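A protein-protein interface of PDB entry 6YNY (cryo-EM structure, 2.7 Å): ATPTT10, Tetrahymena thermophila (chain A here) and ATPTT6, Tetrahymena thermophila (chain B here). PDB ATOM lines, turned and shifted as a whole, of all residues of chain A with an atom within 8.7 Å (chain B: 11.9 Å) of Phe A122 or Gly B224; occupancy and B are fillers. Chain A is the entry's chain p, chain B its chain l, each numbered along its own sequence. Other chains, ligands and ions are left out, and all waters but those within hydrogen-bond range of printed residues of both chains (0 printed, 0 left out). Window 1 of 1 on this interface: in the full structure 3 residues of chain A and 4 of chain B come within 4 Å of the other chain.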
ATOM      1  N   LEU A 117     -22.599 -30.086  -0.999  1.00  0.00           N
ATOM      2  CA  LEU A 117     -22.081 -29.351   0.146  1.00  0.00           C
ATOM      3  C   LEU A 117     -22.966 -28.165   0.496  1.00  0.00           C
ATOM      4  O   LEU A 117     -23.101 -27.818   1.675  1.00  0.00           O
ATOM      5  CB  LEU A 117     -20.659 -28.885  -0.146  1.00  0.00           C
ATOM      6  CG  LEU A 117     -19.830 -28.420   1.043  1.00  0.00           C
ATOM      7  CD1 LEU A 117     -19.509 -29.583   1.944  1.00  0.00           C
ATOM      8  CD2 LEU A 117     -18.568 -27.765   0.560  1.00  0.00           C
ATOM      9  N   SER A 118     -23.578 -27.539  -0.506  1.00  0.00           N
ATOM     10  CA  SER A 118     -24.463 -26.409  -0.275  1.00  0.00           C
ATOM     11  C   SER A 118     -25.809 -26.819   0.305  1.00  0.00           C
ATOM     12  O   SER A 118     -26.608 -25.940   0.642  1.00  0.00           O
ATOM     13  CB  SER A 118     -24.680 -25.655  -1.583  1.00  0.00           C
ATOM     14  OG  SER A 118     -25.611 -24.605  -1.411  1.00  0.00           O
ATOM     15  N   LYS A 119     -26.076 -28.116   0.433  1.00  0.00           N
ATOM     16  CA  LYS A 119     -27.345 -28.612   0.940  1.00  0.00           C
ATOM     17  C   LYS A 119     -27.218 -29.293   2.293  1.00  0.00           C
ATOM     18  O   LYS A 119     -28.225 -29.763   2.830  1.00  0.00           O
ATOM     19  CB  LYS A 119     -27.963 -29.591  -0.060  1.00  0.00           C
ATOM     20  CG  LYS A 119     -28.153 -29.036  -1.452  1.00  0.00           C
ATOM     21  CD  LYS A 119     -29.222 -27.979  -1.486  1.00  0.00           C
ATOM     22  CE  LYS A 119     -29.449 -27.477  -2.895  1.00  0.00           C
ATOM     23  NZ  LYS A 119     -29.856 -28.568  -3.809  1.00  0.00           N
ATOM     24  N   LEU A 120     -26.016 -29.372   2.849  1.00  0.00           N
ATOM     25  CA  LEU A 120     -25.811 -30.041   4.122  1.00  0.00           C
ATOM     26  C   LEU A 120     -26.170 -29.123   5.280  1.00  0.00           C
ATOM     27  O   LEU A 120     -26.066 -27.897   5.189  1.00  0.00           O
ATOM     28  CB  LEU A 120     -24.363 -30.497   4.264  1.00  0.00           C
ATOM     29  CG  LEU A 120     -23.916 -31.619   3.334  1.00  0.00           C
ATOM     30  CD1 LEU A 120     -22.445 -31.859   3.496  1.00  0.00           C
ATOM     31  CD2 LEU A 120     -24.681 -32.883   3.623  1.00  0.00           C
ATOM     32  N   TYR A 121     -26.592 -29.735   6.380  1.00  0.00           N
ATOM     33  CA  TYR A 121     -26.937 -29.001   7.584  1.00  0.00           C
ATOM     34  C   TYR A 121     -25.686 -28.752   8.410  1.00  0.00           C
ATOM     35  O   TYR A 121     -24.836 -29.635   8.555  1.00  0.00           O
ATOM     36  CB  TYR A 121     -27.964 -29.772   8.409  1.00  0.00           C
ATOM     37  CG  TYR A 121     -28.568 -28.977   9.536  1.00  0.00           C
ATOM     38  CD1 TYR A 121     -29.660 -28.158   9.315  1.00  0.00           C
ATOM     39  CD2 TYR A 121     -28.056 -29.050  10.818  1.00  0.00           C
ATOM     40  CE1 TYR A 121     -30.221 -27.432  10.335  1.00  0.00           C
ATOM     41  CE2 TYR A 121     -28.611 -28.325  11.846  1.00  0.00           C
ATOM     42  CZ  TYR A 121     -29.694 -27.518  11.599  1.00  0.00           C
ATOM     43  OH  TYR A 121     -30.251 -26.794  12.621  1.00  0.00           O
ATOM     44  N   PHE A 122     -25.575 -27.541   8.940  1.00  0.00           N
ATOM     45  CA  PHE A 122     -24.426 -27.171   9.744  1.00  0.00           C
ATOM     46  C   PHE A 122     -24.863 -26.145  10.774  1.00  0.00           C
ATOM     47  O   PHE A 122     -25.944 -25.558  10.683  1.00  0.00           O
ATOM     48  CB  PHE A 122     -23.285 -26.634   8.879  1.00  0.00           C
ATOM     49  CG  PHE A 122     -23.574 -25.311   8.239  1.00  0.00           C
ATOM     50  CD1 PHE A 122     -23.168 -24.137   8.839  1.00  0.00           C
ATOM     51  CD2 PHE A 122     -24.237 -25.239   7.033  1.00  0.00           C
ATOM     52  CE1 PHE A 122     -23.426 -22.924   8.254  1.00  0.00           C
ATOM     53  CE2 PHE A 122     -24.495 -24.026   6.446  1.00  0.00           C
ATOM     54  CZ  PHE A 122     -24.087 -22.870   7.054  1.00  0.00           C
ATOM     55  N   PHE A 123     -24.007 -25.943  11.769  1.00  0.00           N
ATOM     56  CA  PHE A 123     -24.274 -25.001  12.839  1.00  0.00           C
ATOM     57  C   PHE A 123     -22.990 -24.259  13.166  1.00  0.00           C
ATOM     58  O   PHE A 123     -21.894 -24.657  12.766  1.00  0.00           O
ATOM     59  CB  PHE A 123     -24.824 -25.708  14.079  1.00  0.00           C
ATOM     60  CG  PHE A 123     -23.773 -26.356  14.923  1.00  0.00           C
ATOM     61  CD1 PHE A 123     -22.950 -27.332  14.400  1.00  0.00           C
ATOM     62  CD2 PHE A 123     -23.617 -26.000  16.245  1.00  0.00           C
ATOM     63  CE1 PHE A 123     -21.990 -27.927  15.175  1.00  0.00           C
ATOM     64  CE2 PHE A 123     -22.658 -26.593  17.024  1.00  0.00           C
ATOM     65  CZ  PHE A 123     -21.844 -27.560  16.487  1.00  0.00           C
ATOM     66  N   LEU A 124     -23.140 -23.162  13.899  1.00  0.00           N
ATOM     67  CA  LEU A 124     -22.010 -22.350  14.328  1.00  0.00           C
ATOM     68  C   LEU A 124     -21.587 -22.827  15.710  1.00  0.00           C
ATOM     69  O   LEU A 124     -22.293 -22.602  16.697  1.00  0.00           O
ATOM     70  CB  LEU A 124     -22.387 -20.874  14.331  1.00  0.00           C
ATOM     71  CG  LEU A 124     -23.035 -20.388  13.035  1.00  0.00           C
ATOM     72  CD1 LEU A 124     -23.389 -18.928  13.117  1.00  0.00           C
ATOM     73  CD2 LEU A 124     -22.126 -20.634  11.863  1.00  0.00           C
ATOM     74  N   ASP A 125     -20.435 -23.486  15.778  1.00  0.00           N
ATOM     75  CA  ASP A 125     -19.976 -24.123  17.006  1.00  0.00           C
ATOM     76  C   ASP A 125     -19.431 -23.065  17.957  1.00  0.00           C
ATOM     77  O   ASP A 125     -18.402 -22.442  17.683  1.00  0.00           O
ATOM     78  CB  ASP A 125     -18.917 -25.171  16.685  1.00  0.00           C
ATOM     79  CG  ASP A 125     -18.584 -26.046  17.872  1.00  0.00           C
ATOM     80  OD1 ASP A 125     -19.116 -25.789  18.972  1.00  0.00           O
ATOM     81  OD2 ASP A 125     -17.791 -26.995  17.702  1.00  0.00           O
ATOM     82  N   PHE A 130     -17.383 -20.103  16.916  1.00  0.00           N
ATOM     83  CA  PHE A 130     -18.566 -19.982  16.068  1.00  0.00           C
ATOM     84  C   PHE A 130     -18.253 -20.282  14.608  1.00  0.00           C
ATOM     85  O   PHE A 130     -18.857 -19.704  13.703  1.00  0.00           O
ATOM     86  CB  PHE A 130     -19.203 -18.600  16.203  1.00  0.00           C
ATOM     87  CG  PHE A 130     -19.707 -18.303  17.579  1.00  0.00           C
ATOM     88  CD1 PHE A 130     -18.980 -17.509  18.440  1.00  0.00           C
ATOM     89  CD2 PHE A 130     -20.907 -18.828  18.015  1.00  0.00           C
ATOM     90  CE1 PHE A 130     -19.442 -17.240  19.706  1.00  0.00           C
ATOM     91  CE2 PHE A 130     -21.371 -18.559  19.279  1.00  0.00           C
ATOM     92  CZ  PHE A 130     -20.640 -17.766  20.125  1.00  0.00           C
ATOM     93  N   LYS A 131     -17.313 -21.180  14.369  1.00  0.00           N
ATOM     94  CA  LYS A 131     -17.061 -21.613  13.010  1.00  0.00           C
ATOM     95  C   LYS A 131     -18.137 -22.600  12.571  1.00  0.00           C
ATOM     96  O   LYS A 131     -18.678 -23.346  13.391  1.00  0.00           O
ATOM     97  CB  LYS A 131     -15.694 -22.273  12.901  1.00  0.00           C
ATOM     98  CG  LYS A 131     -14.524 -21.327  13.023  1.00  0.00           C
ATOM     99  CD  LYS A 131     -13.237 -21.998  12.574  1.00  0.00           C
ATOM    100  CE  LYS A 131     -12.023 -21.124  12.829  1.00  0.00           C
ATOM    101  NZ  LYS A 131     -11.789 -20.908  14.283  1.00  0.00           N
ATOM    102  N   PRO A 132     -18.471 -22.625  11.284  1.00  0.00           N
ATOM    103  CA  PRO A 132     -19.454 -23.599  10.806  1.00  0.00           C
ATOM    104  C   PRO A 132     -18.919 -25.017  10.899  1.00  0.00           C
ATOM    105  O   PRO A 132     -17.775 -25.297  10.535  1.00  0.00           O
ATOM    106  CB  PRO A 132     -19.692 -23.180   9.352  1.00  0.00           C
ATOM    107  CG  PRO A 132     -18.482 -22.441   8.972  1.00  0.00           C
ATOM    108  CD  PRO A 132     -17.998 -21.752  10.199  1.00  0.00           C
ATOM    109  N   SER A 133     -19.764 -25.917  11.396  1.00  0.00           N
ATOM    110  CA  SER A 133     -19.373 -27.296  11.627  1.00  0.00           C
ATOM    111  C   SER A 133     -20.473 -28.234  11.159  1.00  0.00           C
ATOM    112  O   SER A 133     -21.659 -27.962  11.356  1.00  0.00           O
ATOM    113  CB  SER A 133     -19.082 -27.544  13.108  1.00  0.00           C
ATOM    114  OG  SER A 133     -18.729 -28.892  13.342  1.00  0.00           O
ATOM    115  N   LEU A 134     -20.067 -29.335  10.531  1.00  0.00           N
ATOM    116  CA  LEU A 134     -21.003 -30.387  10.167  1.00  0.00           C
ATOM    117  C   LEU A 134     -21.340 -31.294  11.339  1.00  0.00           C
ATOM    118  O   LEU A 134     -22.378 -31.961  11.311  1.00  0.00           O
ATOM    119  CB  LEU A 134     -20.426 -31.234   9.036  1.00  0.00           C
ATOM    120  CG  LEU A 134     -20.184 -30.543   7.699  1.00  0.00           C
ATOM    121  CD1 LEU A 134     -19.417 -31.457   6.783  1.00  0.00           C
ATOM    122  CD2 LEU A 134     -21.487 -30.142   7.059  1.00  0.00           C
ATOM    123  N   ASN A 135     -20.488 -31.331  12.363  1.00  0.00           N
ATOM    124  CA  ASN A 135     -20.667 -32.228  13.501  1.00  0.00           C
ATOM    125  C   ASN A 135     -21.640 -31.599  14.496  1.00  0.00           C
ATOM    126  O   ASN A 135     -21.298 -31.251  15.629  1.00  0.00           O
ATOM    127  CB  ASN A 135     -19.324 -32.529  14.150  1.00  0.00           C
ATOM    128  CG  ASN A 135     -18.233 -32.794  13.135  1.00  0.00           C
ATOM    129  OD1 ASN A 135     -17.149 -32.220  13.210  1.00  0.00           O
ATOM    130  ND2 ASN A 135     -18.515 -33.660  12.176  1.00  0.00           N
ATOM    131  N   HIS A 136     -22.882 -31.451  14.050  1.00  0.00           N
ATOM    132  CA  HIS A 136     -23.899 -30.866  14.904  1.00  0.00           C
ATOM    133  C   HIS A 136     -24.374 -31.880  15.938  1.00  0.00           C
ATOM    134  O   HIS A 136     -24.105 -33.081  15.852  1.00  0.00           O
ATOM    135  CB  HIS A 136     -25.067 -30.335  14.075  1.00  0.00           C
ATOM    136  CG  HIS A 136     -25.658 -31.336  13.137  1.00  0.00           C
ATOM    137  ND1 HIS A 136     -26.585 -32.273  13.535  1.00  0.00           N
ATOM    138  CD2 HIS A 136     -25.462 -31.538  11.814  1.00  0.00           C
ATOM    139  CE1 HIS A 136     -26.930 -33.013  12.499  1.00  0.00           C
ATOM    140  NE2 HIS A 136     -26.263 -32.588  11.443  1.00  0.00           N
ATOM    141  N   HIS A 137     -25.095 -31.375  16.935  1.00  0.00           N
ATOM    142  CA  HIS A 137     -25.484 -32.162  18.096  1.00  0.00           C
ATOM    143  C   HIS A 137     -26.489 -33.254  17.779  1.00  0.00           C
ATOM    144  O   HIS A 137     -26.858 -34.007  18.686  1.00  0.00           O
ATOM    145  CB  HIS A 137     -26.040 -31.234  19.171  1.00  0.00           C
ATOM    146  CG  HIS A 137     -25.014 -30.319  19.757  1.00  0.00           C
ATOM    147  ND1 HIS A 137     -24.383 -29.341  19.020  1.00  0.00           N
ATOM    148  CD2 HIS A 137     -24.495 -30.244  21.004  1.00  0.00           C
ATOM    149  CE1 HIS A 137     -23.526 -28.697  19.792  1.00  0.00           C
ATOM    150  NE2 HIS A 137     -23.575 -29.226  21.000  1.00  0.00           N
ATOM    151  N   VAL A 139     -25.731 -35.331  15.133  1.00  0.00           N
ATOM    152  CA  VAL A 139     -24.912 -36.276  14.387  1.00  0.00           C
ATOM    153  C   VAL A 139     -24.621 -37.490  15.254  1.00  0.00           C
ATOM    154  O   VAL A 139     -24.509 -37.395  16.481  1.00  0.00           O
ATOM    155  CB  VAL A 139     -23.612 -35.596  13.915  1.00  0.00           C
ATOM    156  CG1 VAL A 139     -22.707 -36.590  13.240  1.00  0.00           C
ATOM    157  CG2 VAL A 139     -23.930 -34.463  12.982  1.00  0.00           C
ATOM    158  N   ARG A 143     -19.554 -39.561   8.063  1.00  0.00           N
ATOM    159  CA  ARG A 143     -19.842 -39.507   6.631  1.00  0.00           C
ATOM    160  C   ARG A 143     -19.387 -40.763   5.895  1.00  0.00           C
ATOM    161  O   ARG A 143     -20.191 -41.426   5.234  1.00  0.00           O
ATOM    162  CB  ARG A 143     -19.181 -38.262   6.034  1.00  0.00           C
ATOM    163  CG  ARG A 143     -19.569 -36.973   6.743  1.00  0.00           C
ATOM    164  CD  ARG A 143     -21.011 -36.589   6.486  1.00  0.00           C
ATOM    165  NE  ARG A 143     -21.455 -35.526   7.382  1.00  0.00           N
ATOM    166  CZ  ARG A 143     -22.659 -34.969   7.345  1.00  0.00           C
ATOM    167  NH1 ARG A 143     -23.554 -35.364   6.450  1.00  0.00           N
ATOM    168  NH2 ARG A 143     -22.967 -34.012   8.207  1.00  0.00           N
ATOM    169  N   ALA B 220     -29.877 -15.425  -1.017  1.00  0.00           N
ATOM    170  CA  ALA B 220     -29.466 -15.203   0.365  1.00  0.00           C
ATOM    171  C   ALA B 220     -28.939 -16.526   0.898  1.00  0.00           C
ATOM    172  O   ALA B 220     -29.712 -17.396   1.307  1.00  0.00           O
ATOM    173  CB  ALA B 220     -30.624 -14.678   1.201  1.00  0.00           C
ATOM    174  N   HIS B 221     -27.621 -16.678   0.886  1.00  0.00           N
ATOM    175  CA  HIS B 221     -27.010 -17.931   1.299  1.00  0.00           C
ATOM    176  C   HIS B 221     -27.095 -18.098   2.809  1.00  0.00           C
ATOM    177  O   HIS B 221     -26.685 -17.216   3.569  1.00  0.00           O
ATOM    178  CB  HIS B 221     -25.561 -17.984   0.835  1.00  0.00           C
ATOM    179  CG  HIS B 221     -25.406 -17.928  -0.651  1.00  0.00           C
ATOM    180  ND1 HIS B 221     -25.462 -19.051  -1.446  1.00  0.00           N
ATOM    181  CD2 HIS B 221     -25.210 -16.883  -1.487  1.00  0.00           C
ATOM    182  CE1 HIS B 221     -25.300 -18.700  -2.709  1.00  0.00           C
ATOM    183  NE2 HIS B 221     -25.144 -17.391  -2.761  1.00  0.00           N
ATOM    184  N   TRP B 222     -27.625 -19.238   3.236  1.00  0.00           N
ATOM    185  CA  TRP B 222     -27.807 -19.511   4.653  1.00  0.00           C
ATOM    186  C   TRP B 222     -26.472 -19.480   5.382  1.00  0.00           C
ATOM    187  O   TRP B 222     -25.500 -20.110   4.955  1.00  0.00           O
ATOM    188  CB  TRP B 222     -28.480 -20.869   4.821  1.00  0.00           C
ATOM    189  CG  TRP B 222     -28.911 -21.186   6.202  1.00  0.00           C
ATOM    190  CD1 TRP B 222     -29.582 -20.370   7.057  1.00  0.00           C
ATOM    191  CD2 TRP B 222     -28.726 -22.422   6.887  1.00  0.00           C
ATOM    192  NE1 TRP B 222     -29.820 -21.018   8.239  1.00  0.00           N
ATOM    193  CE2 TRP B 222     -29.302 -22.283   8.160  1.00  0.00           C
ATOM    194  CE3 TRP B 222     -28.123 -23.633   6.551  1.00  0.00           C
ATOM    195  CZ2 TRP B 222     -29.292 -23.308   9.095  1.00  0.00           C
ATOM    196  CZ3 TRP B 222     -28.115 -24.646   7.478  1.00  0.00           C
ATOM    197  CH2 TRP B 222     -28.696 -24.478   8.735  1.00  0.00           C
ATOM    198  N   ASP B 223     -26.430 -18.740   6.488  1.00  0.00           N
ATOM    199  CA  ASP B 223     -25.231 -18.591   7.297  1.00  0.00           C
ATOM    200  C   ASP B 223     -25.251 -19.448   8.554  1.00  0.00           C
ATOM    201  O   ASP B 223     -24.370 -19.301   9.405  1.00  0.00           O
ATOM    202  CB  ASP B 223     -25.037 -17.125   7.679  1.00  0.00           C
ATOM    203  CG  ASP B 223     -26.166 -16.588   8.531  1.00  0.00           C
ATOM    204  OD1 ASP B 223     -27.149 -17.322   8.751  1.00  0.00           O
ATOM    205  OD2 ASP B 223     -26.068 -15.430   8.984  1.00  0.00           O
ATOM    206  N   GLY B 224     -26.234 -20.329   8.697  1.00  0.00           N
ATOM    207  CA  GLY B 224     -26.322 -21.195   9.848  1.00  0.00           C
ATOM    208  C   GLY B 224     -27.210 -20.696  10.960  1.00  0.00           C
ATOM    209  O   GLY B 224     -27.199 -21.283  12.046  1.00  0.00           O
ATOM    210  N   THR B 225     -27.982 -19.642  10.725  1.00  0.00           N
ATOM    211  CA  THR B 225     -28.830 -19.034  11.734  1.00  0.00           C
ATOM    212  C   THR B 225     -30.289 -19.121  11.311  1.00  0.00           C
ATOM    213  O   THR B 225     -30.618 -19.458  10.171  1.00  0.00           O
ATOM    214  CB  THR B 225     -28.446 -17.571  11.974  1.00  0.00           C
ATOM    215  OG1 THR B 225     -28.594 -16.828  10.760  1.00  0.00           O
ATOM    216  CG2 THR B 225     -27.022 -17.474  12.449  1.00  0.00           C
ATOM    217  N   GLN B 226     -31.164 -18.814  12.265  1.00  0.00           N
ATOM    218  CA  GLN B 226     -32.601 -18.763  12.039  1.00  0.00           C
ATOM    219  C   GLN B 226     -33.147 -17.347  12.150  1.00  0.00           C
ATOM    220  O   GLN B 226     -34.358 -17.162  12.300  1.00  0.00           O
ATOM    221  CB  GLN B 226     -33.315 -19.686  13.024  1.00  0.00           C
ATOM    222  CG  GLN B 226     -32.985 -21.143  12.845  1.00  0.00           C
ATOM    223  CD  GLN B 226     -33.525 -21.696  11.551  1.00  0.00           C
ATOM    224  OE1 GLN B 226     -34.547 -21.238  11.048  1.00  0.00           O
ATOM    225  NE2 GLN B 226     -32.836 -22.682  10.998  1.00  0.00           N
ATOM    226  N   ASN B 227     -32.274 -16.341  12.073  1.00  0.00           N
ATOM    227  CA  ASN B 227     -32.664 -14.952  12.281  1.00  0.00           C
ATOM    228  C   ASN B 227     -32.100 -14.027  11.211  1.00  0.00           C
ATOM    229  O   ASN B 227     -32.028 -12.814  11.428  1.00  0.00           O
ATOM    230  CB  ASN B 227     -32.207 -14.486  13.662  1.00  0.00           C
ATOM    231  CG  ASN B 227     -30.725 -14.664  13.874  1.00  0.00           C
ATOM    232  OD1 ASN B 227     -29.945 -14.696  12.925  1.00  0.00           O
ATOM    233  ND2 ASN B 227     -30.326 -14.788  15.125  1.00  0.00           N
ATOM    234  N   MET B 228     -31.707 -14.564  10.064  1.00  0.00           N
ATOM    235  CA  MET B 228     -31.133 -13.754   9.000  1.00  0.00           C
ATOM    236  C   MET B 228     -32.114 -12.671   8.571  1.00  0.00           C
ATOM    237  O   MET B 228     -33.175 -12.982   8.018  1.00  0.00           O
ATOM    238  CB  MET B 228     -30.761 -14.621   7.801  1.00  0.00           C
ATOM    239  CG  MET B 228     -29.713 -15.664   8.096  1.00  0.00           C
ATOM    240  SD  MET B 228     -29.320 -16.680   6.665  1.00  0.00           S
ATOM    241  CE  MET B 228     -28.593 -15.455   5.591  1.00  0.00           C
ATOM    242  N   PRO B 229     -31.803 -11.395   8.797  1.00  0.00           N
ATOM    243  CA  PRO B 229     -32.723 -10.325   8.375  1.00  0.00           C
ATOM    244  C   PRO B 229     -32.608 -10.026   6.886  1.00  0.00           C
ATOM    245  O   PRO B 229     -32.141  -8.973   6.447  1.00  0.00           O
ATOM    246  CB  PRO B 229     -32.282  -9.154   9.255  1.00  0.00           C
ATOM    247  CG  PRO B 229     -30.843  -9.374   9.435  1.00  0.00           C
ATOM    248  CD  PRO B 229     -30.634 -10.849   9.505  1.00  0.00           C
ATOM    249  N   ILE B 230     -33.047 -10.990   6.075  1.00  0.00           N
ATOM    250  CA  ILE B 230     -33.019 -10.825   4.625  1.00  0.00           C
ATOM    251  C   ILE B 230     -34.154  -9.956   4.116  1.00  0.00           C
ATOM    252  O   ILE B 230     -34.179  -9.618   2.926  1.00  0.00           O
ATOM    253  CB  ILE B 230     -33.044 -12.196   3.929  1.00  0.00           C
ATOM    254  CG1 ILE B 230     -34.246 -13.018   4.389  1.00  0.00           C
ATOM    255  CG2 ILE B 230     -31.764 -12.936   4.215  1.00  0.00           C
ATOM    256  CD1 ILE B 230     -34.418 -14.303   3.634  1.00  0.00           C
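The backbone carbonyl oxygen (O) of Thr B225 sits at hydrogen-bond distance from the indole nitrogen (NE1) of Trp B222, at 2.6 Å. The side-chain carboxylate of Asp B223 is in hydrogen-bond range of the side-chain hydroxyl of Thr B225. N of Asp B223 is in hydrogen-bond range of SD of Met B228, 3.6 Å away. OG1 of Thr B225 is in hydrogen-bond range of OD1 of Asn B227.
CE1 of Tyr A121 touches CH2 of Trp B222, at 3.7 Å. Phe A122 touches Trp B222 (O to CH2, 3.5 Å). Phe A122 touches Asp B223 (CZ to C, 3.9 Å). CZ of Phe A122 touches N of Gly B224 (3.7 Å). Leu A124 touches Asp B223. Leu A124 touches Thr B225 (CD1 to CG2, 3.97 Å).
Leu A117 touches none of the printed residues of chain B. No residue of chain B comes within 4 Å of Leu A120. Of chain B, only Trp B222 (3.7 Å) comes within 4 Å of Tyr A121. Of the printed residues of chain B, Phe A122 touches Trp B222, Asp B223 and Gly B224. No residue of chain B comes within 4 Å of Phe A123. Of the printed residues of chain B, Leu A124 touches Asp B223 and Thr B225. No residue of chain B comes within 4 Å of Pro A132. No residue of chain B comes within 4 Å of Leu A134. Of the printed residues of chain A, Trp B222 touches Tyr A121 and Phe A122. Printed residues of chain A within 4 Å of Asp B223: Phe A122 (3.9 Å) and Leu A124 (3.6 Å). Of chain A, only Phe A122 comes within 4 Å of Gly B224. Printed residues of chain A within 4 Å of Thr B225: Leu A124. Pro B229 touches none of the printed residues of chain A. The nearest residue of chain B that does not touch Phe A122 is Thr B225 (6.1 Å). The nearest residue of chain A that does not touch Gly B224 is Leu A124 (4.4 Å).
Hydrophobic or aromatic side chains of chain B within 4 Å of the printed part of chain A: Trp B222. Along chain B the printed residues that touch a printed residue of chain A span positions 222 to 225. Among the printed residues, no Asp or Glu carboxylate lies within 4 Å of a Lys or Arg side-chain nitrogen of the other chain.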
